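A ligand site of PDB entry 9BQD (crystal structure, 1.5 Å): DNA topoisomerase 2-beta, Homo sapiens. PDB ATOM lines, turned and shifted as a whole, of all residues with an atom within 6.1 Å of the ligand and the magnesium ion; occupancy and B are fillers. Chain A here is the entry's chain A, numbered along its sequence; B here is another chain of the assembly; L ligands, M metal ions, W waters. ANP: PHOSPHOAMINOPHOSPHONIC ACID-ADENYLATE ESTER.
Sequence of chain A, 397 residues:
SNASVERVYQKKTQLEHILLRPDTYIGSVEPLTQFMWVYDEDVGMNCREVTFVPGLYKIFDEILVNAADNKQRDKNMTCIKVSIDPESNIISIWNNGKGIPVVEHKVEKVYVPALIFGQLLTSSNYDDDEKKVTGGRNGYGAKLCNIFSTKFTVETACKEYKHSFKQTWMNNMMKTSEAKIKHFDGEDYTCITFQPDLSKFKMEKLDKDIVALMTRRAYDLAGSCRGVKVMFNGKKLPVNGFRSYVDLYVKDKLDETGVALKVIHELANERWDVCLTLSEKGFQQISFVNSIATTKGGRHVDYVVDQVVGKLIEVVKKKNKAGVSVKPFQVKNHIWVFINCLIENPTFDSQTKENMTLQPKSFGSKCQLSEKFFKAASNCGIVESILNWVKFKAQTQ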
ATOM      1  N   GLU A  62      -1.760  -0.256  -0.627  1.00  0.00           N
ATOM      2  CA  GLU A  62      -0.643   0.541  -1.130  1.00  0.00           C
ATOM      3  C   GLU A  62      -1.036   1.319  -2.370  1.00  0.00           C
ATOM      4  O   GLU A  62      -0.669   2.494  -2.533  1.00  0.00           O
ATOM      5  CB  GLU A  62       0.563  -0.344  -1.394  1.00  0.00           C
ATOM      6  CG  GLU A  62       1.178  -0.967  -0.121  1.00  0.00           C
ATOM      7  CD  GLU A  62       1.898   0.007   0.820  1.00  0.00           C
ATOM      8  OE1 GLU A  62       2.026   1.214   0.516  1.00  0.00           O
ATOM      9  OE2 GLU A  62       2.352  -0.468   1.898  1.00  0.00           O
ATOM     10  N   ILE A  63      -1.769   0.678  -3.285  1.00  0.00           N
ATOM     11  CA  ILE A  63      -2.155   1.337  -4.519  1.00  0.00           C
ATOM     12  C   ILE A  63      -3.225   2.393  -4.258  1.00  0.00           C
ATOM     13  O   ILE A  63      -3.217   3.482  -4.851  1.00  0.00           O
ATOM     14  CB  ILE A  63      -2.580   0.276  -5.564  1.00  0.00           C
ATOM     15  CG1 ILE A  63      -1.473  -0.764  -5.771  1.00  0.00           C
ATOM     16  CG2 ILE A  63      -2.993   0.960  -6.845  1.00  0.00           C
ATOM     17  CD1 ILE A  63      -0.110  -0.193  -6.158  1.00  0.00           C
ATOM     18  N   VAL A  65      -3.725   4.189  -1.418  1.00  0.00           N
ATOM     19  CA  VAL A  65      -3.140   5.363  -0.788  1.00  0.00           C
ATOM     20  C   VAL A  65      -2.275   6.118  -1.791  1.00  0.00           C
ATOM     21  O   VAL A  65      -2.243   7.352  -1.768  1.00  0.00           O
ATOM     22  CB  VAL A  65      -2.332   4.936   0.465  1.00  0.00           C
ATOM     23  CG1 VAL A  65      -1.564   6.119   1.063  1.00  0.00           C
ATOM     24  CG2 VAL A  65      -3.282   4.345   1.548  1.00  0.00           C
ATOM     25  N   ASN A  66      -1.605   5.417  -2.706  1.00  0.00           N
ATOM     26  CA  ASN A  66      -0.862   6.125  -3.752  1.00  0.00           C
ATOM     27  C   ASN A  66      -1.792   7.021  -4.574  1.00  0.00           C
ATOM     28  O   ASN A  66      -1.394   8.105  -5.032  1.00  0.00           O
ATOM     29  CB  ASN A  66      -0.158   5.151  -4.689  1.00  0.00           C
ATOM     30  CG  ASN A  66       1.116   4.591  -4.106  1.00  0.00           C
ATOM     31  OD1 ASN A  66       1.646   5.091  -3.118  1.00  0.00           O
ATOM     32  ND2 ASN A  66       1.623   3.544  -4.746  1.00  0.00           N
ATOM     33  N   ALA A  67      -3.013   6.542  -4.852  1.00  0.00           N
ATOM     34  CA  ALA A  67      -3.942   7.379  -5.601  1.00  0.00           C
ATOM     35  C   ALA A  67      -4.331   8.607  -4.776  1.00  0.00           C
ATOM     36  O   ALA A  67      -4.380   9.722  -5.300  1.00  0.00           O
ATOM     37  CB  ALA A  67      -5.175   6.562  -5.998  1.00  0.00           C
ATOM     38  N   ASP A  69      -2.568  10.019  -2.560  1.00  0.00           N
ATOM     39  CA  ASP A  69      -1.390  10.868  -2.481  1.00  0.00           C
ATOM     40  C   ASP A  69      -1.304  11.805  -3.673  1.00  0.00           C
ATOM     41  O   ASP A  69      -0.665  12.864  -3.606  1.00  0.00           O
ATOM     42  CB  ASP A  69      -0.125  10.004  -2.437  1.00  0.00           C
ATOM     43  CG  ASP A  69       0.138   9.402  -1.062  1.00  0.00           C
ATOM     44  OD1 ASP A  69      -0.505   9.820  -0.086  1.00  0.00           O
ATOM     45  OD2 ASP A  69       1.033   8.513  -0.956  1.00  0.00           O
ATOM     46  N   ASN A  70      -1.906  11.417  -4.806  1.00  0.00           N
ATOM     47  CA  ASN A  70      -1.808  12.288  -5.980  1.00  0.00           C
ATOM     48  C   ASN A  70      -2.527  13.608  -5.759  1.00  0.00           C
ATOM     49  O   ASN A  70      -2.238  14.565  -6.476  1.00  0.00           O
ATOM     50  CB  ASN A  70      -2.300  11.602  -7.258  1.00  0.00           C
ATOM     51  CG  ASN A  70      -1.695  12.240  -8.487  1.00  0.00           C
ATOM     52  OD1 ASN A  70      -0.468  12.290  -8.635  1.00  0.00           O
ATOM     53  ND2 ASN A  70      -2.545  12.745  -9.375  1.00  0.00           N
ATOM     54  N   ARG A  73       0.130  16.098  -5.083  1.00  0.00           N
ATOM     55  CA  ARG A  73       0.896  16.510  -6.247  1.00  0.00           C
ATOM     56  C   ARG A  73       0.078  17.421  -7.161  1.00  0.00           C
ATOM     57  O   ARG A  73       0.650  18.230  -7.888  1.00  0.00           O
ATOM     58  CB  ARG A  73       1.244  15.303  -7.122  1.00  0.00           C
ATOM     59  CG  ARG A  73       2.460  14.515  -6.779  1.00  0.00           C
ATOM     60  CD  ARG A  73       2.647  13.464  -7.889  1.00  0.00           C
ATOM     61  NE  ARG A  73       3.143  14.051  -9.139  1.00  0.00           N
ATOM     62  CZ  ARG A  73       2.620  13.847 -10.341  1.00  0.00           C
ATOM     63  NH1 ARG A  73       1.533  13.105 -10.518  1.00  0.00           N
ATOM     64  NH2 ARG A  73       3.224  14.383 -11.405  1.00  0.00           N
ATOM     65  N   ASN A  95      -7.072   7.195 -11.057  1.00  0.00           N
ATOM     66  CA  ASN A  95      -7.189   8.543 -10.503  1.00  0.00           C
ATOM     67  C   ASN A  95      -6.954   9.551 -11.607  1.00  0.00           C
ATOM     68  O   ASN A  95      -6.258   9.277 -12.583  1.00  0.00           O
ATOM     69  CB  ASN A  95      -6.224   8.771  -9.322  1.00  0.00           C
ATOM     70  CG  ASN A  95      -4.766   8.779  -9.747  1.00  0.00           C
ATOM     71  OD1 ASN A  95      -4.082   7.763  -9.694  1.00  0.00           O
ATOM     72  ND2 ASN A  95      -4.286   9.945 -10.163  1.00  0.00           N
ATOM     73  N   LYS A  98      -2.745  15.162 -12.235  1.00  0.00           N
ATOM     74  CA  LYS A  98      -1.546  15.004 -13.047  1.00  0.00           C
ATOM     75  C   LYS A  98      -1.095  13.554 -13.109  1.00  0.00           C
ATOM     76  O   LYS A  98      -1.045  12.845 -12.093  1.00  0.00           O
ATOM     77  CB  LYS A  98      -0.405  15.819 -12.454  1.00  0.00           C
ATOM     78  CG  LYS A  98      -0.351  17.284 -12.812  1.00  0.00           C
ATOM     79  CD  LYS A  98       0.848  17.930 -12.119  1.00  0.00           C
ATOM     80  CE  LYS A  98       0.873  19.451 -12.295  1.00  0.00           C
ATOM     81  NZ  LYS A  98       2.101  20.113 -11.723  1.00  0.00           N
ATOM     82  N   GLY A  99      -0.729  13.115 -14.307  1.00  0.00           N
ATOM     83  CA  GLY A  99      -0.083  11.842 -14.483  1.00  0.00           C
ATOM     84  C   GLY A  99       1.380  11.888 -14.065  1.00  0.00           C
ATOM     85  O   GLY A  99       1.877  12.870 -13.502  1.00  0.00           O
ATOM     86  N   ILE A 100       2.076  10.798 -14.346  1.00  0.00           N
ATOM     87  CA  ILE A 100       3.504  10.699 -14.057  1.00  0.00           C
ATOM     88  C   ILE A 100       4.293  11.087 -15.305  1.00  0.00           C
ATOM     89  O   ILE A 100       3.945  10.634 -16.407  1.00  0.00           O
ATOM     90  CB  ILE A 100       3.863   9.281 -13.594  1.00  0.00           C
ATOM     91  CG1 ILE A 100       3.037   8.932 -12.356  1.00  0.00           C
ATOM     92  CG2 ILE A 100       5.346   9.172 -13.271  1.00  0.00           C
ATOM     93  CD1 ILE A 100       2.926   7.472 -12.121  1.00  0.00           C
ATOM     94  N   ILE A 116       9.788   3.798 -10.938  1.00  0.00           N
ATOM     95  CA  ILE A 116       9.112   3.915  -9.655  1.00  0.00           C
ATOM     96  C   ILE A 116       8.093   2.823  -9.415  1.00  0.00           C
ATOM     97  O   ILE A 116       7.619   2.686  -8.270  1.00  0.00           O
ATOM     98  CB  ILE A 116       8.539   5.336  -9.432  1.00  0.00           C
ATOM     99  CG1 ILE A 116       7.357   5.631 -10.365  1.00  0.00           C
ATOM    100  CG2 ILE A 116       9.659   6.386  -9.602  1.00  0.00           C
ATOM    101  CD1 ILE A 116       6.885   7.090 -10.322  1.00  0.00           C
ATOM    102  N   PHE A 117       7.729   2.045 -10.446  1.00  0.00           N
ATOM    103  CA  PHE A 117       6.871   0.864 -10.270  1.00  0.00           C
ATOM    104  C   PHE A 117       7.636  -0.452 -10.397  1.00  0.00           C
ATOM    105  O   PHE A 117       7.099  -1.484 -10.008  1.00  0.00           O
ATOM    106  CB  PHE A 117       5.683   0.860 -11.251  1.00  0.00           C
ATOM    107  CG  PHE A 117       4.625   1.856 -10.904  1.00  0.00           C
ATOM    108  CD1 PHE A 117       3.607   1.543 -10.007  1.00  0.00           C
ATOM    109  CD2 PHE A 117       4.684   3.132 -11.427  1.00  0.00           C
ATOM    110  CE1 PHE A 117       2.667   2.499  -9.644  1.00  0.00           C
ATOM    111  CE2 PHE A 117       3.745   4.092 -11.072  1.00  0.00           C
ATOM    112  CZ  PHE A 117       2.736   3.774 -10.176  1.00  0.00           C
ATOM    113  N   THR A 122      12.349   3.464  -4.580  1.00  0.00           N
ATOM    114  CA  THR A 122      12.159   4.556  -5.518  1.00  0.00           C
ATOM    115  C   THR A 122      10.935   5.352  -5.097  1.00  0.00           C
ATOM    116  O   THR A 122       9.901   4.770  -4.779  1.00  0.00           O
ATOM    117  CB  THR A 122      12.026   4.023  -6.956  1.00  0.00           C
ATOM    118  OG1 THR A 122      10.991   3.031  -7.014  1.00  0.00           O
ATOM    119  CG2 THR A 122      13.352   3.412  -7.443  1.00  0.00           C
ATOM    120  N   SER A 123      11.048   6.678  -5.104  1.00  0.00           N
ATOM    121  CA  SER A 123      10.002   7.485  -4.476  1.00  0.00           C
ATOM    122  C   SER A 123      10.173   8.937  -4.849  1.00  0.00           C
ATOM    123  O   SER A 123      11.287   9.400  -5.121  1.00  0.00           O
ATOM    124  CB  SER A 123      10.103   7.359  -2.954  1.00  0.00           C
ATOM    125  OG  SER A 123       9.063   8.039  -2.279  1.00  0.00           O
ATOM    126  N   SER A 124       9.064   9.667  -4.802  1.00  0.00           N
ATOM    127  CA  SER A 124       9.089  11.127  -4.796  1.00  0.00           C
ATOM    128  C   SER A 124       9.011  11.696  -3.385  1.00  0.00           C
ATOM    129  O   SER A 124       8.929  12.917  -3.217  1.00  0.00           O
ATOM    130  CB  SER A 124       7.967  11.690  -5.656  1.00  0.00           C
ATOM    131  OG  SER A 124       6.695  11.284  -5.149  1.00  0.00           O
ATOM    132  N   ASN A 125       9.046  10.829  -2.360  1.00  0.00           N
ATOM    133  CA  ASN A 125       8.860  11.221  -0.968  1.00  0.00           C
ATOM    134  C   ASN A 125      10.123  11.098  -0.130  1.00  0.00           C
ATOM    135  O   ASN A 125      10.035  10.984   1.096  1.00  0.00           O
ATOM    136  CB  ASN A 125       7.734  10.403  -0.354  1.00  0.00           C
ATOM    137  CG  ASN A 125       6.408  10.779  -0.932  1.00  0.00           C
ATOM    138  OD1 ASN A 125       5.966  11.903  -0.775  1.00  0.00           O
ATOM    139  ND2 ASN A 125       5.777   9.855  -1.638  1.00  0.00           N
ATOM    140  N   GLY A 135       0.756   9.974   2.290  1.00  0.00           N
ATOM    141  CA  GLY A 135       0.980   8.752   3.036  1.00  0.00           C
ATOM    142  C   GLY A 135       2.255   8.044   2.657  1.00  0.00           C
ATOM    143  O   GLY A 135       2.846   7.345   3.483  1.00  0.00           O
ATOM    144  N   GLY A 136       2.711   8.212   1.415  1.00  0.00           N
ATOM    145  CA  GLY A 136       3.923   7.551   0.962  1.00  0.00           C
ATOM    146  C   GLY A 136       5.177   8.140   1.603  1.00  0.00           C
ATOM    147  O   GLY A 136       5.338   9.360   1.709  1.00  0.00           O
ATOM    148  N   ARG A 137       6.068   7.236   2.039  1.00  0.00           N
ATOM    149  CA  ARG A 137       7.315   7.637   2.689  1.00  0.00           C
ATOM    150  C   ARG A 137       8.512   6.790   2.277  1.00  0.00           C
ATOM    151  O   ARG A 137       9.633   7.305   2.310  1.00  0.00           O
ATOM    152  CB  ARG A 137       7.181   7.501   4.205  1.00  0.00           C
ATOM    153  CG  ARG A 137       5.994   8.221   4.794  1.00  0.00           C
ATOM    154  CD  ARG A 137       6.175   9.731   4.739  1.00  0.00           C
ATOM    155  NE  ARG A 137       7.254  10.177   5.608  1.00  0.00           N
ATOM    156  CZ  ARG A 137       8.261  10.954   5.227  1.00  0.00           C
ATOM    157  NH1 ARG A 137       8.262  11.558   4.053  1.00  0.00           N
ATOM    158  NH2 ARG A 137       9.288  11.141   6.049  1.00  0.00           N
ATOM    159  N   ASN A 138       8.327   5.515   1.918  1.00  0.00           N
ATOM    160  CA  ASN A 138       9.429   4.587   1.930  1.00  0.00           C
ATOM    161  C   ASN A 138       9.924   4.127   0.564  1.00  0.00           C
ATOM    162  O   ASN A 138      11.032   3.569   0.501  1.00  0.00           O
ATOM    163  CB  ASN A 138       9.040   3.335   2.733  1.00  0.00           C
ATOM    164  CG  ASN A 138       8.682   3.677   4.152  1.00  0.00           C
ATOM    165  OD1 ASN A 138       9.284   4.568   4.754  1.00  0.00           O
ATOM    166  ND2 ASN A 138       7.675   2.994   4.680  1.00  0.00           N
ATOM    167  N   GLY A 139       9.149   4.299  -0.509  1.00  0.00           N
ATOM    168  CA  GLY A 139       9.586   3.845  -1.814  1.00  0.00           C
ATOM    169  C   GLY A 139       9.439   2.362  -2.070  1.00  0.00           C
ATOM    170  O   GLY A 139      10.162   1.811  -2.919  1.00  0.00           O
ATOM    171  N   TYR A 140       8.489   1.711  -1.392  1.00  0.00           N
ATOM    172  CA  TYR A 140       8.220   0.276  -1.544  1.00  0.00           C
ATOM    173  C   TYR A 140       6.839  -0.061  -2.084  1.00  0.00           C
ATOM    174  O   TYR A 140       6.692  -1.032  -2.814  1.00  0.00           O
ATOM    175  CB  TYR A 140       8.312  -0.427  -0.195  1.00  0.00           C
ATOM    176  CG  TYR A 140       9.654  -0.951   0.226  1.00  0.00           C
ATOM    177  CD1 TYR A 140      10.285  -1.963  -0.485  1.00  0.00           C
ATOM    178  CD2 TYR A 140      10.259  -0.496   1.376  1.00  0.00           C
ATOM    179  CE1 TYR A 140      11.495  -2.474  -0.084  1.00  0.00           C
ATOM    180  CE2 TYR A 140      11.495  -1.005   1.792  1.00  0.00           C
ATOM    181  CZ  TYR A 140      12.089  -1.991   1.045  1.00  0.00           C
ATOM    182  OH  TYR A 140      13.309  -2.541   1.409  1.00  0.00           O
ATOM    183  N   GLY A 141       5.800   0.678  -1.667  1.00  0.00           N
ATOM    184  CA  GLY A 141       4.430   0.153  -1.741  1.00  0.00           C
ATOM    185  C   GLY A 141       4.018  -0.413  -3.080  1.00  0.00           C
ATOM    186  O   GLY A 141       3.467  -1.518  -3.157  1.00  0.00           O
ATOM    187  N   ALA A 142       4.241   0.351  -4.155  1.00  0.00           N
ATOM    188  CA  ALA A 142       3.801  -0.102  -5.462  1.00  0.00           C
ATOM    189  C   ALA A 142       4.594  -1.314  -5.924  1.00  0.00           C
ATOM    190  O   ALA A 142       4.059  -2.190  -6.611  1.00  0.00           O
ATOM    191  CB  ALA A 142       3.936   1.025  -6.505  1.00  0.00           C
ATOM    192  N   LYS A 143       5.892  -1.362  -5.605  1.00  0.00           N
ATOM    193  CA  LYS A 143       6.673  -2.530  -5.985  1.00  0.00           C
ATOM    194  C   LYS A 143       6.197  -3.765  -5.217  1.00  0.00           C
ATOM    195  O   LYS A 143       6.143  -4.857  -5.781  1.00  0.00           O
ATOM    196  CB  LYS A 143       8.159  -2.298  -5.728  1.00  0.00           C
ATOM    197  CG  LYS A 143       8.893  -1.530  -6.836  1.00  0.00           C
ATOM    198  CD  LYS A 143       8.529  -0.023  -6.871  1.00  0.00           C
ATOM    199  CE  LYS A 143       8.946   0.721  -5.621  1.00  0.00           C
ATOM    200  NZ  LYS A 143       8.568   2.160  -5.762  1.00  0.00           N
ATOM    201  N   THR A 156      -0.345   5.507 -17.499  1.00  0.00           N
ATOM    202  CA  THR A 156      -0.351   6.890 -17.028  1.00  0.00           C
ATOM    203  C   THR A 156      -0.216   7.816 -18.230  1.00  0.00           C
ATOM    204  O   THR A 156       0.441   7.471 -19.218  1.00  0.00           O
ATOM    205  CB  THR A 156       0.732   7.128 -15.961  1.00  0.00           C
ATOM    206  OG1 THR A 156       0.553   8.416 -15.362  1.00  0.00           O
ATOM    207  CG2 THR A 156       2.119   7.083 -16.556  1.00  0.00           C
ATOM    208  N   THR A 190      -3.896   8.246 -14.082  1.00  0.00           N
ATOM    209  CA  THR A 190      -3.086   7.064 -13.856  1.00  0.00           C
ATOM    210  C   THR A 190      -4.038   5.922 -13.489  1.00  0.00           C
ATOM    211  O   THR A 190      -4.994   6.124 -12.754  1.00  0.00           O
ATOM    212  CB  THR A 190      -2.059   7.270 -12.733  1.00  0.00           C
ATOM    213  OG1 THR A 190      -1.119   8.268 -13.127  1.00  0.00           O
ATOM    214  CG2 THR A 190      -1.294   5.986 -12.423  1.00  0.00           C
ATOM    215  N   ILE A 192      -3.777   1.787 -12.320  1.00  0.00           N
ATOM    216  CA  ILE A 192      -3.024   0.612 -11.934  1.00  0.00           C
ATOM    217  C   ILE A 192      -4.002  -0.542 -11.933  1.00  0.00           C
ATOM    218  O   ILE A 192      -5.020  -0.492 -11.223  1.00  0.00           O
ATOM    219  CB  ILE A 192      -2.406   0.782 -10.541  1.00  0.00           C
ATOM    220  CG1 ILE A 192      -1.587   2.087 -10.453  1.00  0.00           C
ATOM    221  CG2 ILE A 192      -1.579  -0.443 -10.169  1.00  0.00           C
ATOM    222  CD1 ILE A 192      -0.559   2.268 -11.534  1.00  0.00           C
ATOM    223  N   GLN A 351       6.250  -0.927   7.494  1.00  0.00           N
ATOM    224  CA  GLN A 351       5.741  -0.545   6.176  1.00  0.00           C
ATOM    225  C   GLN A 351       4.223  -0.582   6.126  1.00  0.00           C
ATOM    226  O   GLN A 351       3.613   0.157   5.347  1.00  0.00           O
ATOM    227  CB  GLN A 351       6.310  -1.484   5.097  1.00  0.00           C
ATOM    228  CG  GLN A 351       5.723  -1.275   3.712  1.00  0.00           C
ATOM    229  CD  GLN A 351       6.157   0.027   3.065  1.00  0.00           C
ATOM    230  OE1 GLN A 351       7.242   0.547   3.346  1.00  0.00           O
ATOM    231  NE2 GLN A 351       5.314   0.564   2.179  1.00  0.00           N
ATOM    232  N   LYS A 353       2.199   0.486   8.294  1.00  0.00           N
ATOM    233  CA  LYS A 353       1.710   1.801   8.742  1.00  0.00           C
ATOM    234  C   LYS A 353       0.474   1.722   9.627  1.00  0.00           C
ATOM    235  O   LYS A 353      -0.408   2.586   9.556  1.00  0.00           O
ATOM    236  CB  LYS A 353       1.480   2.726   7.546  1.00  0.00           C
ATOM    237  CG  LYS A 353       2.760   3.010   6.783  1.00  0.00           C
ATOM    238  CD  LYS A 353       2.478   3.822   5.546  1.00  0.00           C
ATOM    239  CE  LYS A 353       3.646   3.723   4.593  1.00  0.00           C
ATOM    240  NZ  LYS A 353       3.393   4.505   3.357  1.00  0.00           N
ATOM    241  N   TYR B   9      12.119  12.421  -8.420  1.00  0.00           N
ATOM    242  CA  TYR B   9      12.063  10.939  -8.395  1.00  0.00           C
ATOM    243  C   TYR B   9      13.465  10.409  -8.112  1.00  0.00           C
ATOM    244  O   TYR B   9      14.364  10.547  -8.941  1.00  0.00           O
ATOM    245  CB  TYR B   9      11.497  10.401  -9.706  1.00  0.00           C
ATOM    246  CG  TYR B   9      10.095  10.883  -9.965  1.00  0.00           C
ATOM    247  CD1 TYR B   9       9.000  10.293  -9.342  1.00  0.00           C
ATOM    248  CD2 TYR B   9       9.848  11.973 -10.801  1.00  0.00           C
ATOM    249  CE1 TYR B   9       7.722  10.740  -9.548  1.00  0.00           C
ATOM    250  CE2 TYR B   9       8.548  12.426 -11.018  1.00  0.00           C
ATOM    251  CZ  TYR B   9       7.496  11.805 -10.382  1.00  0.00           C
ATOM    252  OH  TYR B   9       6.217  12.248 -10.579  1.00  0.00           O
HETATM  253  PG  ANP L   1       5.551   3.966   0.324  1.00  0.00           P
HETATM  254  O1G ANP L   1       4.177   3.776  -0.242  1.00  0.00           O
HETATM  255  O2G ANP L   1       6.467   2.706   0.159  1.00  0.00           O
HETATM  256  O3G ANP L   1       5.578   4.437   1.814  1.00  0.00           O
HETATM  257  PB  ANP L   1       5.830   5.791  -1.981  1.00  0.00           P
HETATM  258  O1B ANP L   1       4.358   5.973  -2.153  1.00  0.00           O
HETATM  259  O2B ANP L   1       6.607   7.068  -2.310  1.00  0.00           O
HETATM  260  N3B ANP L   1       6.286   5.324  -0.443  1.00  0.00           N
HETATM  261  PA  ANP L   1       5.472   3.729  -3.931  1.00  0.00           P
HETATM  262  O1A ANP L   1       6.282   2.551  -4.301  1.00  0.00           O
HETATM  263  O2A ANP L   1       4.112   3.434  -3.311  1.00  0.00           O
HETATM  264  O3A ANP L   1       6.330   4.626  -2.920  1.00  0.00           O
HETATM  265  O5' ANP L   1       5.241   4.660  -5.168  1.00  0.00           O
HETATM  266  C5' ANP L   1       6.424   5.074  -5.898  1.00  0.00           C
HETATM  267  C4' ANP L   1       6.210   6.448  -6.473  1.00  0.00           C
HETATM  268  O4' ANP L   1       5.310   6.352  -7.593  1.00  0.00           O
HETATM  269  C3' ANP L   1       5.560   7.458  -5.525  1.00  0.00           C
HETATM  270  O3' ANP L   1       6.570   8.066  -4.727  1.00  0.00           O
HETATM  271  C2' ANP L   1       4.904   8.432  -6.506  1.00  0.00           C
HETATM  272  O2' ANP L   1       5.830   9.417  -6.962  1.00  0.00           O
HETATM  273  C1' ANP L   1       4.555   7.547  -7.699  1.00  0.00           C
HETATM  274  N9  ANP L   1       3.138   7.175  -7.800  1.00  0.00           N
HETATM  275  C8  ANP L   1       2.561   6.012  -7.350  1.00  0.00           C
HETATM  276  N7  ANP L   1       1.277   5.943  -7.596  1.00  0.00           N
HETATM  277  C5  ANP L   1       0.991   7.134  -8.253  1.00  0.00           C
HETATM  278  C6  ANP L   1      -0.199   7.666  -8.774  1.00  0.00           C
HETATM  279  N6  ANP L   1      -1.384   7.051  -8.702  1.00  0.00           N
HETATM  280  N1  ANP L   1      -0.138   8.878  -9.376  1.00  0.00           N
HETATM  281  C2  ANP L   1       1.051   9.501  -9.444  1.00  0.00           C
HETATM  282  N3  ANP L   1       2.236   9.099  -8.979  1.00  0.00           N
HETATM  283  C4  ANP L   1       2.144   7.897  -8.386  1.00  0.00           C
HETATM  284 MG    MG M   1       3.047   4.392  -1.787  1.00  0.00          MG
HETATM  285  O   HOH W   1       0.184   3.287  -7.399  1.00  0.00           O
HETATM  286  O   HOH W   2       1.530  11.163  -6.397  1.00  0.00           O
HETATM  287  O   HOH W   3       1.386   8.678  -5.382  1.00  0.00           O
HETATM  288  O   HOH W   4      -2.398   4.422  -7.466  1.00  0.00           O
HETATM  289  O   HOH W   5       4.284  11.048  -9.184  1.00  0.00           O
HETATM  290  O   HOH W   6       1.283   3.624   1.694  1.00  0.00           O
HETATM  291  O   HOH W   7       2.750   8.179  -3.049  1.00  0.00           O
HETATM  292  O   HOH W   8       1.848   2.771  -1.555  1.00  0.00           O
HETATM  293  O   HOH W   9       1.809   5.521  -0.383  1.00  0.00           O
HETATM  294  O   HOH W  10      -1.571  10.200 -11.378  1.00  0.00           O
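Of the 33 residues printed, 1 comes within 4 Å of the magnesium ion.
NZ of Lys 353 is in hydrogen-bond range of O of Gly 135.
The side-chain amino group (NZ) of Lys 143 sits close to the backbone carbonyl oxygen (O) of Gly 139, 3.3 Å away.
OG1 of Thr 122 sits at hydrogen-bond distance from NZ of Lys 143.
N of Asn 95 sits at hydrogen-bond distance from O of Thr 190 (2.9 Å).
The side-chain amide nitrogen of Gln 351 is in hydrogen-bond range of the side-chain carboxylate of Glu 62 (3.1 Å).
The guanidinium group (NH1) of Arg 73 sits at hydrogen-bond distance from the side-chain amide oxygen (OD1) of Asn 70, 2.9 Å away.
O of Lys 98 lies within hydrogen-bond range of NH1 of Arg 73.
OG1 of Thr 156 is in hydrogen-bond range of OG1 of Thr 190, 2.8 Å away.
Water W8 bridges the side-chain carboxylate (OE1) of Glu 62 and the side-chain amide nitrogen (ND2) of Asn 66.
Water W10 lies within hydrogen-bond range of OG1 of Thr 190 (2.6 Å), O of Lys 98 (2.8 Å), N1 of the ligand (2.8 Å), ND2 of Asn 95 (3.0 Å) and ND2 of Asn 70 (3.4 Å).
Water W1 bridges a nitrogen (N7) of the ligand (2.9 Å) and the side-chain amide nitrogen (ND2) of Asn 66 (3.0 Å).
Water W4 lies within hydrogen-bond range of the backbone carbonyl oxygen (O) of Ile 63 (2.9 Å), a nitrogen (N6) of the ligand (3.1 Å) and the backbone NH (N) of Ala 67 (3.4 Å).
Water W2 lies within hydrogen-bond range of the side-chain amide oxygen (OD1) of Asn 70 (3.2 Å) and a nitrogen (N3) of the ligand (3.4 Å).
Water W6 lies within hydrogen-bond range of the side-chain carboxylate of Glu 62 and the side-chain amino group of Lys 353.
The side-chain hydroxyl (OG) of Ser 123 sits at hydrogen-bond distance from an oxygen (O2B) of the ligand (2.6 Å).
NZ of Lys 353 lies within salt-bridge range of O3G of the ligand (2.7 Å).
N of Tyr 140 lies within hydrogen-bond range of O2G of the ligand (2.7 Å).
The side-chain amino group of Lys 143 lies within salt-bridge range of an oxygen (O1A) of the ligand (2.7 Å).
The backbone NH (N) of Ser 124 sits at hydrogen-bond distance from an oxygen (O3') of the ligand.
The side-chain hydroxyl of Ser 124 sits at hydrogen-bond distance from an oxygen (O2') of the ligand (2.7 Å).
The backbone NH (N) of Gly 141 sits at hydrogen-bond distance from an oxygen (O2G) of the ligand (2.8 Å).
The backbone NH of Arg 137 is in hydrogen-bond range of an oxygen (O3G) of the ligand, 2.9 Å away.
O3G of the ligand sits at hydrogen-bond distance from N of Asn 138.
A nitrogen (N6) of the ligand lies within hydrogen-bond range of the side-chain amide oxygen of Asn 95 (3.0 Å).
An oxygen (O2B) of the ligand is in hydrogen-bond range of the side-chain amide nitrogen of Asn 125, at 3.0 Å.
An oxygen (O1A) of the ligand sits at hydrogen-bond distance from the backbone NH of Ala 142, at 3.0 Å.
The backbone NH of Gly 139 lies within hydrogen-bond range of an oxygen (O2G) of the ligand (3.2 Å).
The side-chain amide nitrogen (NE2) of Gln 351 is in hydrogen-bond range of an oxygen (O2G) of the ligand (3.2 Å).
OE1 of Glu 62 sits close to O1G of the ligand, at 3.4 Å.
Asn 70 touches the ligand (OD1 to C2, 3.3 Å).
Arg 73 touches the ligand (NH1 to C2, 3.8 Å).
Ile 100 touches the ligand (CG1 to N3, 3.5 Å).
Ile 116 touches the ligand (CD1 to O4', 3.2 Å).
Phe 117 touches the ligand (CZ to C8, 3.6 Å).
Thr 122 touches the ligand.
Gly 136 touches the ligand.
Thr 190 touches the ligand (CG2 to N6, 3.9 Å).
CE1 of Tyr 9 of chain B touches O2' of the ligand (3.5 Å).
Hydrophobic or aromatic side chains within 4 Å of the ligand: Ile 100, Ile 116, Phe 117, Tyr 140, Ala 142 and Tyr 9 of chain B.
Along chain A the residues within 4 Å of the ligand span positions 62 to 353.
The magnesium ion is bound by O1G of the ligand (2.0 Å), water W8 (2.0 Å), OD1 of Asn 66 (2.1 Å), O1B of the ligand (2.1 Å), O2A of the ligand (2.1 Å) and water W9 (2.2 Å).
The magnesium ion has six donor atoms within binding distance.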
